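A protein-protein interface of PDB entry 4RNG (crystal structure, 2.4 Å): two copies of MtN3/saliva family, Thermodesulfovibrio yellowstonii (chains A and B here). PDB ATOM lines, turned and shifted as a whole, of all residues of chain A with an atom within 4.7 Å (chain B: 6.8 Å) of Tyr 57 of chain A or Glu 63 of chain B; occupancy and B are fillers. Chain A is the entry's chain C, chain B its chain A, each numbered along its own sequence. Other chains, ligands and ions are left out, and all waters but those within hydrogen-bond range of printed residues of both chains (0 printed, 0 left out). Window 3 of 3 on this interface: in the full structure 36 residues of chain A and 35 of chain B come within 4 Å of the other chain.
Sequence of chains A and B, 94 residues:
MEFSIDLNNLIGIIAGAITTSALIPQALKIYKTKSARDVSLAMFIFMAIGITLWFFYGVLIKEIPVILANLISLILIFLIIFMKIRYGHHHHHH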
ATOM      1  N   LEU A  53     -36.292  36.288  23.877  1.00  0.00           N
ATOM      2  CA  LEU A  53     -35.459  35.787  24.973  1.00  0.00           C
ATOM      3  C   LEU A  53     -34.473  34.699  24.531  1.00  0.00           C
ATOM      4  O   LEU A  53     -33.359  34.637  25.023  1.00  0.00           O
ATOM      5  CB  LEU A  53     -36.333  35.261  26.106  1.00  0.00           C
ATOM      6  CG  LEU A  53     -36.896  36.331  27.026  1.00  0.00           C
ATOM      7  CD1 LEU A  53     -37.714  35.707  28.151  1.00  0.00           C
ATOM      8  CD2 LEU A  53     -35.720  37.082  27.603  1.00  0.00           C
ATOM      9  N   TRP A  54     -34.886  33.824  23.617  1.00  0.00           N
ATOM     10  CA  TRP A  54     -33.959  32.843  23.061  1.00  0.00           C
ATOM     11  C   TRP A  54     -32.798  33.556  22.354  1.00  0.00           C
ATOM     12  O   TRP A  54     -31.656  33.116  22.409  1.00  0.00           O
ATOM     13  CB  TRP A  54     -34.674  31.924  22.077  1.00  0.00           C
ATOM     14  CG  TRP A  54     -35.383  30.796  22.719  1.00  0.00           C
ATOM     15  CD1 TRP A  54     -36.722  30.549  22.685  1.00  0.00           C
ATOM     16  CD2 TRP A  54     -34.804  29.748  23.498  1.00  0.00           C
ATOM     17  NE1 TRP A  54     -37.010  29.413  23.390  1.00  0.00           N
ATOM     18  CE2 TRP A  54     -35.834  28.901  23.912  1.00  0.00           C
ATOM     19  CE3 TRP A  54     -33.492  29.444  23.894  1.00  0.00           C
ATOM     20  CZ2 TRP A  54     -35.624  27.763  24.689  1.00  0.00           C
ATOM     21  CZ3 TRP A  54     -33.275  28.325  24.675  1.00  0.00           C
ATOM     22  CH2 TRP A  54     -34.336  27.496  25.063  1.00  0.00           C
ATOM     23  N   PHE A  55     -33.103  34.665  21.687  1.00  0.00           N
ATOM     24  CA  PHE A  55     -32.066  35.487  21.096  1.00  0.00           C
ATOM     25  C   PHE A  55     -31.028  35.949  22.123  1.00  0.00           C
ATOM     26  O   PHE A  55     -29.836  35.765  21.923  1.00  0.00           O
ATOM     27  CB  PHE A  55     -32.682  36.705  20.413  1.00  0.00           C
ATOM     28  CG  PHE A  55     -31.709  37.842  20.241  1.00  0.00           C
ATOM     29  CD1 PHE A  55     -30.692  37.778  19.298  1.00  0.00           C
ATOM     30  CD2 PHE A  55     -31.800  38.969  21.037  1.00  0.00           C
ATOM     31  CE1 PHE A  55     -29.774  38.810  19.150  1.00  0.00           C
ATOM     32  CE2 PHE A  55     -30.890  40.014  20.887  1.00  0.00           C
ATOM     33  CZ  PHE A  55     -29.876  39.932  19.932  1.00  0.00           C
ATOM     34  N   PHE A  56     -31.495  36.539  23.217  1.00  0.00           N
ATOM     35  CA  PHE A  56     -30.628  37.015  24.299  1.00  0.00           C
ATOM     36  C   PHE A  56     -29.763  35.891  24.826  1.00  0.00           C
ATOM     37  O   PHE A  56     -28.546  36.033  24.995  1.00  0.00           O
ATOM     38  CB  PHE A  56     -31.480  37.614  25.419  1.00  0.00           C
ATOM     39  CG  PHE A  56     -30.696  38.314  26.491  1.00  0.00           C
ATOM     40  CD1 PHE A  56     -29.565  39.049  26.191  1.00  0.00           C
ATOM     41  CD2 PHE A  56     -31.094  38.233  27.814  1.00  0.00           C
ATOM     42  CE1 PHE A  56     -28.847  39.696  27.188  1.00  0.00           C
ATOM     43  CE2 PHE A  56     -30.375  38.860  28.804  1.00  0.00           C
ATOM     44  CZ  PHE A  56     -29.252  39.598  28.487  1.00  0.00           C
ATOM     45  N   TYR A  57     -30.414  34.767  25.086  1.00  0.00           N
ATOM     46  CA  TYR A  57     -29.754  33.540  25.510  1.00  0.00           C
ATOM     47  C   TYR A  57     -28.622  33.129  24.549  1.00  0.00           C
ATOM     48  O   TYR A  57     -27.527  32.768  24.976  1.00  0.00           O
ATOM     49  CB  TYR A  57     -30.792  32.428  25.586  1.00  0.00           C
ATOM     50  CG  TYR A  57     -30.232  31.078  25.914  1.00  0.00           C
ATOM     51  CD1 TYR A  57     -29.864  30.760  27.212  1.00  0.00           C
ATOM     52  CD2 TYR A  57     -30.042  30.125  24.921  1.00  0.00           C
ATOM     53  CE1 TYR A  57     -29.367  29.516  27.521  1.00  0.00           C
ATOM     54  CE2 TYR A  57     -29.522  28.885  25.219  1.00  0.00           C
ATOM     55  CZ  TYR A  57     -29.192  28.588  26.517  1.00  0.00           C
ATOM     56  OH  TYR A  57     -28.671  27.369  26.823  1.00  0.00           O
ATOM     57  N   GLY A  58     -28.899  33.166  23.249  1.00  0.00           N
ATOM     58  CA  GLY A  58     -27.885  32.825  22.268  1.00  0.00           C
ATOM     59  C   GLY A  58     -26.676  33.749  22.352  1.00  0.00           C
ATOM     60  O   GLY A  58     -25.525  33.347  22.161  1.00  0.00           O
ATOM     61  N   VAL A  59     -26.949  35.016  22.609  1.00  0.00           N
ATOM     62  CA  VAL A  59     -25.896  35.993  22.732  1.00  0.00           C
ATOM     63  C   VAL A  59     -25.032  35.732  23.966  1.00  0.00           C
ATOM     64  O   VAL A  59     -23.817  35.822  23.881  1.00  0.00           O
ATOM     65  CB  VAL A  59     -26.473  37.422  22.762  1.00  0.00           C
ATOM     66  CG1 VAL A  59     -25.387  38.425  23.066  1.00  0.00           C
ATOM     67  CG2 VAL A  59     -27.140  37.740  21.424  1.00  0.00           C
ATOM     68  N   LEU A  60     -25.656  35.409  25.101  1.00  0.00           N
ATOM     69  CA  LEU A  60     -24.908  35.131  26.329  1.00  0.00           C
ATOM     70  C   LEU A  60     -23.981  33.905  26.207  1.00  0.00           C
ATOM     71  O   LEU A  60     -22.820  33.949  26.630  1.00  0.00           O
ATOM     72  CB  LEU A  60     -25.858  34.940  27.514  1.00  0.00           C
ATOM     73  CG  LEU A  60     -26.694  36.133  27.996  1.00  0.00           C
ATOM     74  CD1 LEU A  60     -27.700  35.693  29.040  1.00  0.00           C
ATOM     75  CD2 LEU A  60     -25.848  37.280  28.533  1.00  0.00           C
ATOM     76  N   ILE A  61     -24.497  32.809  25.653  1.00  0.00           N
ATOM     77  CA  ILE A  61     -23.715  31.579  25.487  1.00  0.00           C
ATOM     78  C   ILE A  61     -22.871  31.638  24.206  1.00  0.00           C
ATOM     79  O   ILE A  61     -22.210  30.666  23.841  1.00  0.00           O
ATOM     80  CB  ILE A  61     -24.608  30.312  25.488  1.00  0.00           C
ATOM     81  CG1 ILE A  61     -25.546  30.304  24.282  1.00  0.00           C
ATOM     82  CG2 ILE A  61     -25.418  30.219  26.776  1.00  0.00           C
ATOM     83  CD1 ILE A  61     -26.206  28.957  24.043  1.00  0.00           C
ATOM     84  N   VAL A  66     -28.281  29.888  17.403  1.00  0.00           N
ATOM     85  CA  VAL A  66     -29.382  30.349  18.249  1.00  0.00           C
ATOM     86  C   VAL A  66     -29.730  31.798  17.935  1.00  0.00           C
ATOM     87  O   VAL A  66     -30.900  32.168  17.793  1.00  0.00           O
ATOM     88  CB  VAL A  66     -29.031  30.235  19.729  1.00  0.00           C
ATOM     89  CG1 VAL A  66     -30.245  30.586  20.593  1.00  0.00           C
ATOM     90  CG2 VAL A  66     -28.517  28.849  20.028  1.00  0.00           C
ATOM     91  N   LEU B   7     -26.748  33.144  35.123  1.00  0.00           N
ATOM     92  CA  LEU B   7     -27.495  34.079  34.284  1.00  0.00           C
ATOM     93  C   LEU B   7     -28.019  33.352  33.041  1.00  0.00           C
ATOM     94  O   LEU B   7     -29.182  33.500  32.665  1.00  0.00           O
ATOM     95  CB  LEU B   7     -26.637  35.285  33.897  1.00  0.00           C
ATOM     96  CG  LEU B   7     -27.296  36.278  32.944  1.00  0.00           C
ATOM     97  CD1 LEU B   7     -28.611  36.771  33.524  1.00  0.00           C
ATOM     98  CD2 LEU B   7     -26.355  37.456  32.677  1.00  0.00           C
ATOM     99  N   ASN B   8     -27.144  32.573  32.413  1.00  0.00           N
ATOM    100  CA  ASN B   8     -27.481  31.814  31.211  1.00  0.00           C
ATOM    101  C   ASN B   8     -28.716  30.935  31.376  1.00  0.00           C
ATOM    102  O   ASN B   8     -29.587  30.864  30.485  1.00  0.00           O
ATOM    103  CB  ASN B   8     -26.310  30.922  30.794  1.00  0.00           C
ATOM    104  CG  ASN B   8     -25.087  31.703  30.414  1.00  0.00           C
ATOM    105  OD1 ASN B   8     -25.084  32.933  30.411  1.00  0.00           O
ATOM    106  ND2 ASN B   8     -24.032  30.986  30.067  1.00  0.00           N
ATOM    107  N   ASN B   9     -28.752  30.222  32.495  1.00  0.00           N
ATOM    108  CA  ASN B   9     -29.844  29.316  32.764  1.00  0.00           C
ATOM    109  C   ASN B   9     -31.108  30.089  33.057  1.00  0.00           C
ATOM    110  O   ASN B   9     -32.194  29.676  32.648  1.00  0.00           O
ATOM    111  CB  ASN B   9     -29.494  28.380  33.915  1.00  0.00           C
ATOM    112  CG  ASN B   9     -28.481  27.336  33.512  1.00  0.00           C
ATOM    113  OD1 ASN B   9     -28.332  27.027  32.333  1.00  0.00           O
ATOM    114  ND2 ASN B   9     -27.734  26.832  34.483  1.00  0.00           N
ATOM    115  N   LEU B  10     -30.977  31.242  33.701  1.00  0.00           N
ATOM    116  CA  LEU B  10     -32.164  32.049  33.951  1.00  0.00           C
ATOM    117  C   LEU B  10     -32.878  32.407  32.635  1.00  0.00           C
ATOM    118  O   LEU B  10     -34.073  32.184  32.495  1.00  0.00           O
ATOM    119  CB  LEU B  10     -31.808  33.327  34.704  1.00  0.00           C
ATOM    120  CG  LEU B  10     -32.971  34.299  34.957  1.00  0.00           C
ATOM    121  CD1 LEU B  10     -34.064  33.643  35.819  1.00  0.00           C
ATOM    122  CD2 LEU B  10     -32.512  35.628  35.553  1.00  0.00           C
ATOM    123  N   ILE B  11     -32.144  32.956  31.673  1.00  0.00           N
ATOM    124  CA  ILE B  11     -32.755  33.374  30.419  1.00  0.00           C
ATOM    125  C   ILE B  11     -33.229  32.180  29.586  1.00  0.00           C
ATOM    126  O   ILE B  11     -34.316  32.200  28.997  1.00  0.00           O
ATOM    127  CB  ILE B  11     -31.780  34.229  29.597  1.00  0.00           C
ATOM    128  CG1 ILE B  11     -31.200  35.330  30.470  1.00  0.00           C
ATOM    129  CG2 ILE B  11     -32.458  34.780  28.364  1.00  0.00           C
ATOM    130  CD1 ILE B  11     -32.226  36.346  30.907  1.00  0.00           C
ATOM    131  N   GLY B  12     -32.407  31.140  29.526  1.00  0.00           N
ATOM    132  CA  GLY B  12     -32.752  29.989  28.720  1.00  0.00           C
ATOM    133  C   GLY B  12     -34.023  29.330  29.196  1.00  0.00           C
ATOM    134  O   GLY B  12     -34.926  29.035  28.424  1.00  0.00           O
ATOM    135  N   ILE B  13     -34.092  29.116  30.495  1.00  0.00           N
ATOM    136  CA  ILE B  13     -35.224  28.442  31.068  1.00  0.00           C
ATOM    137  C   ILE B  13     -36.451  29.292  30.869  1.00  0.00           C
ATOM    138  O   ILE B  13     -37.498  28.781  30.464  1.00  0.00           O
ATOM    139  CB  ILE B  13     -34.984  28.149  32.551  1.00  0.00           C
ATOM    140  CG1 ILE B  13     -33.888  27.086  32.677  1.00  0.00           C
ATOM    141  CG2 ILE B  13     -36.249  27.693  33.213  1.00  0.00           C
ATOM    142  CD1 ILE B  13     -33.249  27.008  34.034  1.00  0.00           C
ATOM    143  N   ALA B  15     -36.938  31.614  28.562  1.00  0.00           N
ATOM    144  CA  ALA B  15     -37.254  31.506  27.144  1.00  0.00           C
ATOM    145  C   ALA B  15     -37.960  30.196  26.816  1.00  0.00           C
ATOM    146  O   ALA B  15     -38.971  30.181  26.106  1.00  0.00           O
ATOM    147  CB  ALA B  15     -35.993  31.632  26.292  1.00  0.00           C
ATOM    148  N   PHE B  55     -32.944  19.653  19.650  1.00  0.00           N
ATOM    149  CA  PHE B  55     -32.691  18.739  20.766  1.00  0.00           C
ATOM    150  C   PHE B  55     -31.286  18.112  20.659  1.00  0.00           C
ATOM    151  O   PHE B  55     -30.530  18.159  21.626  1.00  0.00           O
ATOM    152  CB  PHE B  55     -33.773  17.667  20.814  1.00  0.00           C
ATOM    153  CG  PHE B  55     -33.444  16.495  21.680  1.00  0.00           C
ATOM    154  CD1 PHE B  55     -33.520  16.591  23.061  1.00  0.00           C
ATOM    155  CD2 PHE B  55     -33.091  15.286  21.116  1.00  0.00           C
ATOM    156  CE1 PHE B  55     -33.231  15.504  23.858  1.00  0.00           C
ATOM    157  CE2 PHE B  55     -32.809  14.188  21.909  1.00  0.00           C
ATOM    158  CZ  PHE B  55     -32.877  14.295  23.285  1.00  0.00           C
ATOM    159  N   TYR B  57     -28.771  19.242  18.984  1.00  0.00           N
ATOM    160  CA  TYR B  57     -27.890  20.380  19.169  1.00  0.00           C
ATOM    161  C   TYR B  57     -27.675  20.686  20.649  1.00  0.00           C
ATOM    162  O   TYR B  57     -26.534  20.856  21.099  1.00  0.00           O
ATOM    163  CB  TYR B  57     -28.462  21.598  18.441  1.00  0.00           C
ATOM    164  CG  TYR B  57     -27.677  22.862  18.631  1.00  0.00           C
ATOM    165  CD1 TYR B  57     -26.463  23.043  17.985  1.00  0.00           C
ATOM    166  CD2 TYR B  57     -28.144  23.881  19.444  1.00  0.00           C
ATOM    167  CE1 TYR B  57     -25.732  24.202  18.145  1.00  0.00           C
ATOM    168  CE2 TYR B  57     -27.424  25.035  19.610  1.00  0.00           C
ATOM    169  CZ  TYR B  57     -26.212  25.189  18.959  1.00  0.00           C
ATOM    170  OH  TYR B  57     -25.471  26.337  19.112  1.00  0.00           O
ATOM    171  N   GLY B  58     -28.767  20.711  21.406  1.00  0.00           N
ATOM    172  CA  GLY B  58     -28.686  21.016  22.819  1.00  0.00           C
ATOM    173  C   GLY B  58     -27.816  20.028  23.562  1.00  0.00           C
ATOM    174  O   GLY B  58     -27.047  20.397  24.448  1.00  0.00           O
ATOM    175  N   VAL B  59     -27.947  18.761  23.194  1.00  0.00           N
ATOM    176  CA  VAL B  59     -27.154  17.710  23.800  1.00  0.00           C
ATOM    177  C   VAL B  59     -25.687  17.876  23.425  1.00  0.00           C
ATOM    178  O   VAL B  59     -24.810  17.741  24.269  1.00  0.00           O
ATOM    179  CB  VAL B  59     -27.649  16.334  23.375  1.00  0.00           C
ATOM    180  CG1 VAL B  59     -26.730  15.293  23.912  1.00  0.00           C
ATOM    181  CG2 VAL B  59     -29.071  16.100  23.885  1.00  0.00           C
ATOM    182  N   LEU B  60     -25.428  18.180  22.157  1.00  0.00           N
ATOM    183  CA  LEU B  60     -24.065  18.396  21.685  1.00  0.00           C
ATOM    184  C   LEU B  60     -23.373  19.576  22.357  1.00  0.00           C
ATOM    185  O   LEU B  60     -22.247  19.450  22.816  1.00  0.00           O
ATOM    186  CB  LEU B  60     -24.064  18.599  20.173  1.00  0.00           C
ATOM    187  CG  LEU B  60     -24.399  17.370  19.342  1.00  0.00           C
ATOM    188  CD1 LEU B  60     -24.602  17.745  17.880  1.00  0.00           C
ATOM    189  CD2 LEU B  60     -23.245  16.402  19.483  1.00  0.00           C
ATOM    190  N   ILE B  61     -24.038  20.720  22.416  1.00  0.00           N
ATOM    191  CA  ILE B  61     -23.437  21.882  23.047  1.00  0.00           C
ATOM    192  C   ILE B  61     -23.683  21.842  24.558  1.00  0.00           C
ATOM    193  O   ILE B  61     -23.288  22.753  25.290  1.00  0.00           O
ATOM    194  CB  ILE B  61     -23.933  23.201  22.452  1.00  0.00           C
ATOM    195  CG1 ILE B  61     -25.383  23.484  22.839  1.00  0.00           C
ATOM    196  CG2 ILE B  61     -23.693  23.219  20.931  1.00  0.00           C
ATOM    197  CD1 ILE B  61     -25.773  24.934  22.563  1.00  0.00           C
ATOM    198  N   LYS B  62     -24.374  20.796  24.997  1.00  0.00           N
ATOM    199  CA  LYS B  62     -24.627  20.538  26.412  1.00  0.00           C
ATOM    200  C   LYS B  62     -25.390  21.639  27.132  1.00  0.00           C
ATOM    201  O   LYS B  62     -25.007  22.071  28.215  1.00  0.00           O
ATOM    202  CB  LYS B  62     -23.299  20.305  27.126  1.00  0.00           C
ATOM    203  CG  LYS B  62     -22.449  19.182  26.562  1.00  0.00           C
ATOM    204  CD  LYS B  62     -21.125  19.152  27.308  1.00  0.00           C
ATOM    205  CE  LYS B  62     -20.189  18.092  26.771  1.00  0.00           C
ATOM    206  NZ  LYS B  62     -18.934  18.004  27.577  1.00  0.00           N
ATOM    207  N   GLU B  63     -26.488  22.080  26.542  1.00  0.00           N
ATOM    208  CA  GLU B  63     -27.315  23.118  27.153  1.00  0.00           C
ATOM    209  C   GLU B  63     -28.644  22.501  27.539  1.00  0.00           C
ATOM    210  O   GLU B  63     -29.474  22.203  26.683  1.00  0.00           O
ATOM    211  CB  GLU B  63     -27.526  24.289  26.196  1.00  0.00           C
ATOM    212  CG  GLU B  63     -26.309  25.156  25.981  1.00  0.00           C
ATOM    213  CD  GLU B  63     -25.863  25.875  27.233  1.00  0.00           C
ATOM    214  OE1 GLU B  63     -26.736  26.300  28.013  1.00  0.00           O
ATOM    215  OE2 GLU B  63     -24.642  26.028  27.432  1.00  0.00           O
ATOM    216  N   ILE B  64     -28.820  22.274  28.836  1.00  0.00           N
ATOM    217  CA  ILE B  64     -30.016  21.630  29.347  1.00  0.00           C
ATOM    218  C   ILE B  64     -31.286  22.421  28.985  1.00  0.00           C
ATOM    219  O   ILE B  64     -32.289  21.811  28.625  1.00  0.00           O
ATOM    220  CB  ILE B  64     -29.939  21.429  30.875  1.00  0.00           C
ATOM    221  CG1 ILE B  64     -28.594  20.803  31.259  1.00  0.00           C
ATOM    222  CG2 ILE B  64     -31.183  20.686  31.407  1.00  0.00           C
ATOM    223  CD1 ILE B  64     -28.425  19.415  30.752  1.00  0.00           C
ATOM    224  N   PRO B  65     -31.255  23.773  29.063  1.00  0.00           N
ATOM    225  CA  PRO B  65     -32.492  24.447  28.654  1.00  0.00           C
ATOM    226  C   PRO B  65     -32.876  24.190  27.206  1.00  0.00           C
ATOM    227  O   PRO B  65     -34.063  24.086  26.922  1.00  0.00           O
ATOM    228  CB  PRO B  65     -32.171  25.924  28.869  1.00  0.00           C
ATOM    229  CG  PRO B  65     -31.221  25.921  29.989  1.00  0.00           C
ATOM    230  CD  PRO B  65     -30.347  24.711  29.745  1.00  0.00           C
ATOM    231  N   VAL B  66     -31.914  24.094  26.297  1.00  0.00           N
ATOM    232  CA  VAL B  66     -32.251  23.734  24.926  1.00  0.00           C
ATOM    233  C   VAL B  66     -32.784  22.295  24.830  1.00  0.00           C
ATOM    234  O   VAL B  66     -33.734  22.026  24.093  1.00  0.00           O
ATOM    235  CB  VAL B  66     -31.054  23.886  23.985  1.00  0.00           C
ATOM    236  CG1 VAL B  66     -31.494  23.692  22.526  1.00  0.00           C
ATOM    237  CG2 VAL B  66     -30.439  25.239  24.167  1.00  0.00           C
ATOM    238  N   ILE B  67     -32.153  21.372  25.553  1.00  0.00           N
ATOM    239  CA  ILE B  67     -32.562  19.971  25.519  1.00  0.00           C
ATOM    240  C   ILE B  67     -33.995  19.804  25.990  1.00  0.00           C
ATOM    241  O   ILE B  67     -34.848  19.292  25.246  1.00  0.00           O
ATOM    242  CB  ILE B  67     -31.643  19.092  26.382  1.00  0.00           C
ATOM    243  CG1 ILE B  67     -30.231  19.109  25.808  1.00  0.00           C
ATOM    244  CG2 ILE B  67     -32.158  17.676  26.446  1.00  0.00           C
ATOM    245  CD1 ILE B  67     -29.212  18.466  26.697  1.00  0.00           C
ATOM    246  N   LEU B  68     -34.249  20.246  27.221  1.00  0.00           N
ATOM    247  CA  LEU B  68     -35.555  20.076  27.850  1.00  0.00           C
ATOM    248  C   LEU B  68     -36.691  20.841  27.146  1.00  0.00           C
ATOM    249  O   LEU B  68     -37.784  20.286  26.965  1.00  0.00           O
ATOM    250  CB  LEU B  68     -35.514  20.475  29.315  1.00  0.00           C
ATOM    251  CG  LEU B  68     -36.832  20.052  29.958  1.00  0.00           C
ATOM    252  CD1 LEU B  68     -37.016  18.550  29.809  1.00  0.00           C
ATOM    253  CD2 LEU B  68     -36.939  20.472  31.390  1.00  0.00           C
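Of the 21 printed residues of chain B, 9 touch a printed residue of chain A. Of the 10 printed residues of chain A, 7 touch a printed residue of chain B. Hydrophobic or aromatic side chains of chain A within 4 Å of the printed part of chain B: Leu 53, Trp 54, Phe 56, Tyr 57, Leu 60, Ile 61 and Val 66.
The indole nitrogen (NE1) of Trp 54 of chain A is in hydrogen-bond range of the backbone carbonyl oxygen (O) of Ala 15 of chain B (3.4 Å). The side-chain carboxylate (OE1) of Glu 63 of chain B is in hydrogen-bond range of the side-chain hydroxyl (OH) of Tyr 57 of chain A.
The backbone NH (N) of Glu 63 of chain B is in hydrogen-bond range of the backbone carbonyl oxygen (O) of Gly 58 of chain B, at 2.7 Å.
Tyr 57 of chain A touches Val 66 of chain B, and with the chains exchanged Val 66 of chain A touches Tyr 57 of chain B. 7 positions are printed for both chains. Of the 16 pairs that touch across the chains among the printed residues, 2 have their exchanged pair printed and touching as well.
Ile 11 of chain B touches Leu 53 of chain A. CB of Leu 53 of chain A touches CB of Ala 15 of chain B (3.6 Å). Gly 12 of chain B touches Trp 54 of chain A (O to CH2, 3.7 Å). Pro 65 of chain B touches Trp 54 of chain A. CA of Gly 12 of chain B touches CD1 of Tyr 57 of chain A (3.3 Å). Tyr 57 of chain A touches Val 66 of chain B. Leu 60 of chain A touches Asn 8 of chain B. Leu 60 of chain A touches Ile 11 of chain B. CG2 of Ile 61 of chain A touches ND2 of Asn 8 of chain B, 3.7 Å away. Val 66 of chain A touches Tyr 57 of chain B.
Of chain B, only Asn 8, Ile 11, Gly 12, Glu 63 and Val 66 come within 4 Å of Tyr 57 of chain A. Of the printed residues of chain B, Ile 61 of chain A touches Asn 8. Of the printed residues of chain A, Gly 12 of chain B touches Trp 54 and Tyr 57. Printed residues of chain A within 4 Å of Tyr 57 of chain B: Val 66 (3.99 Å). Leu 60 of chain B touches none of the printed residues of chain A. The nearest residue of chain B that does not touch Tyr 57 of chain A is Pro 65 of chain B (4.3 Å). The nearest residue of chain A that does not touch Glu 63 of chain B is Ile 61 of chain A (4.3 Å).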
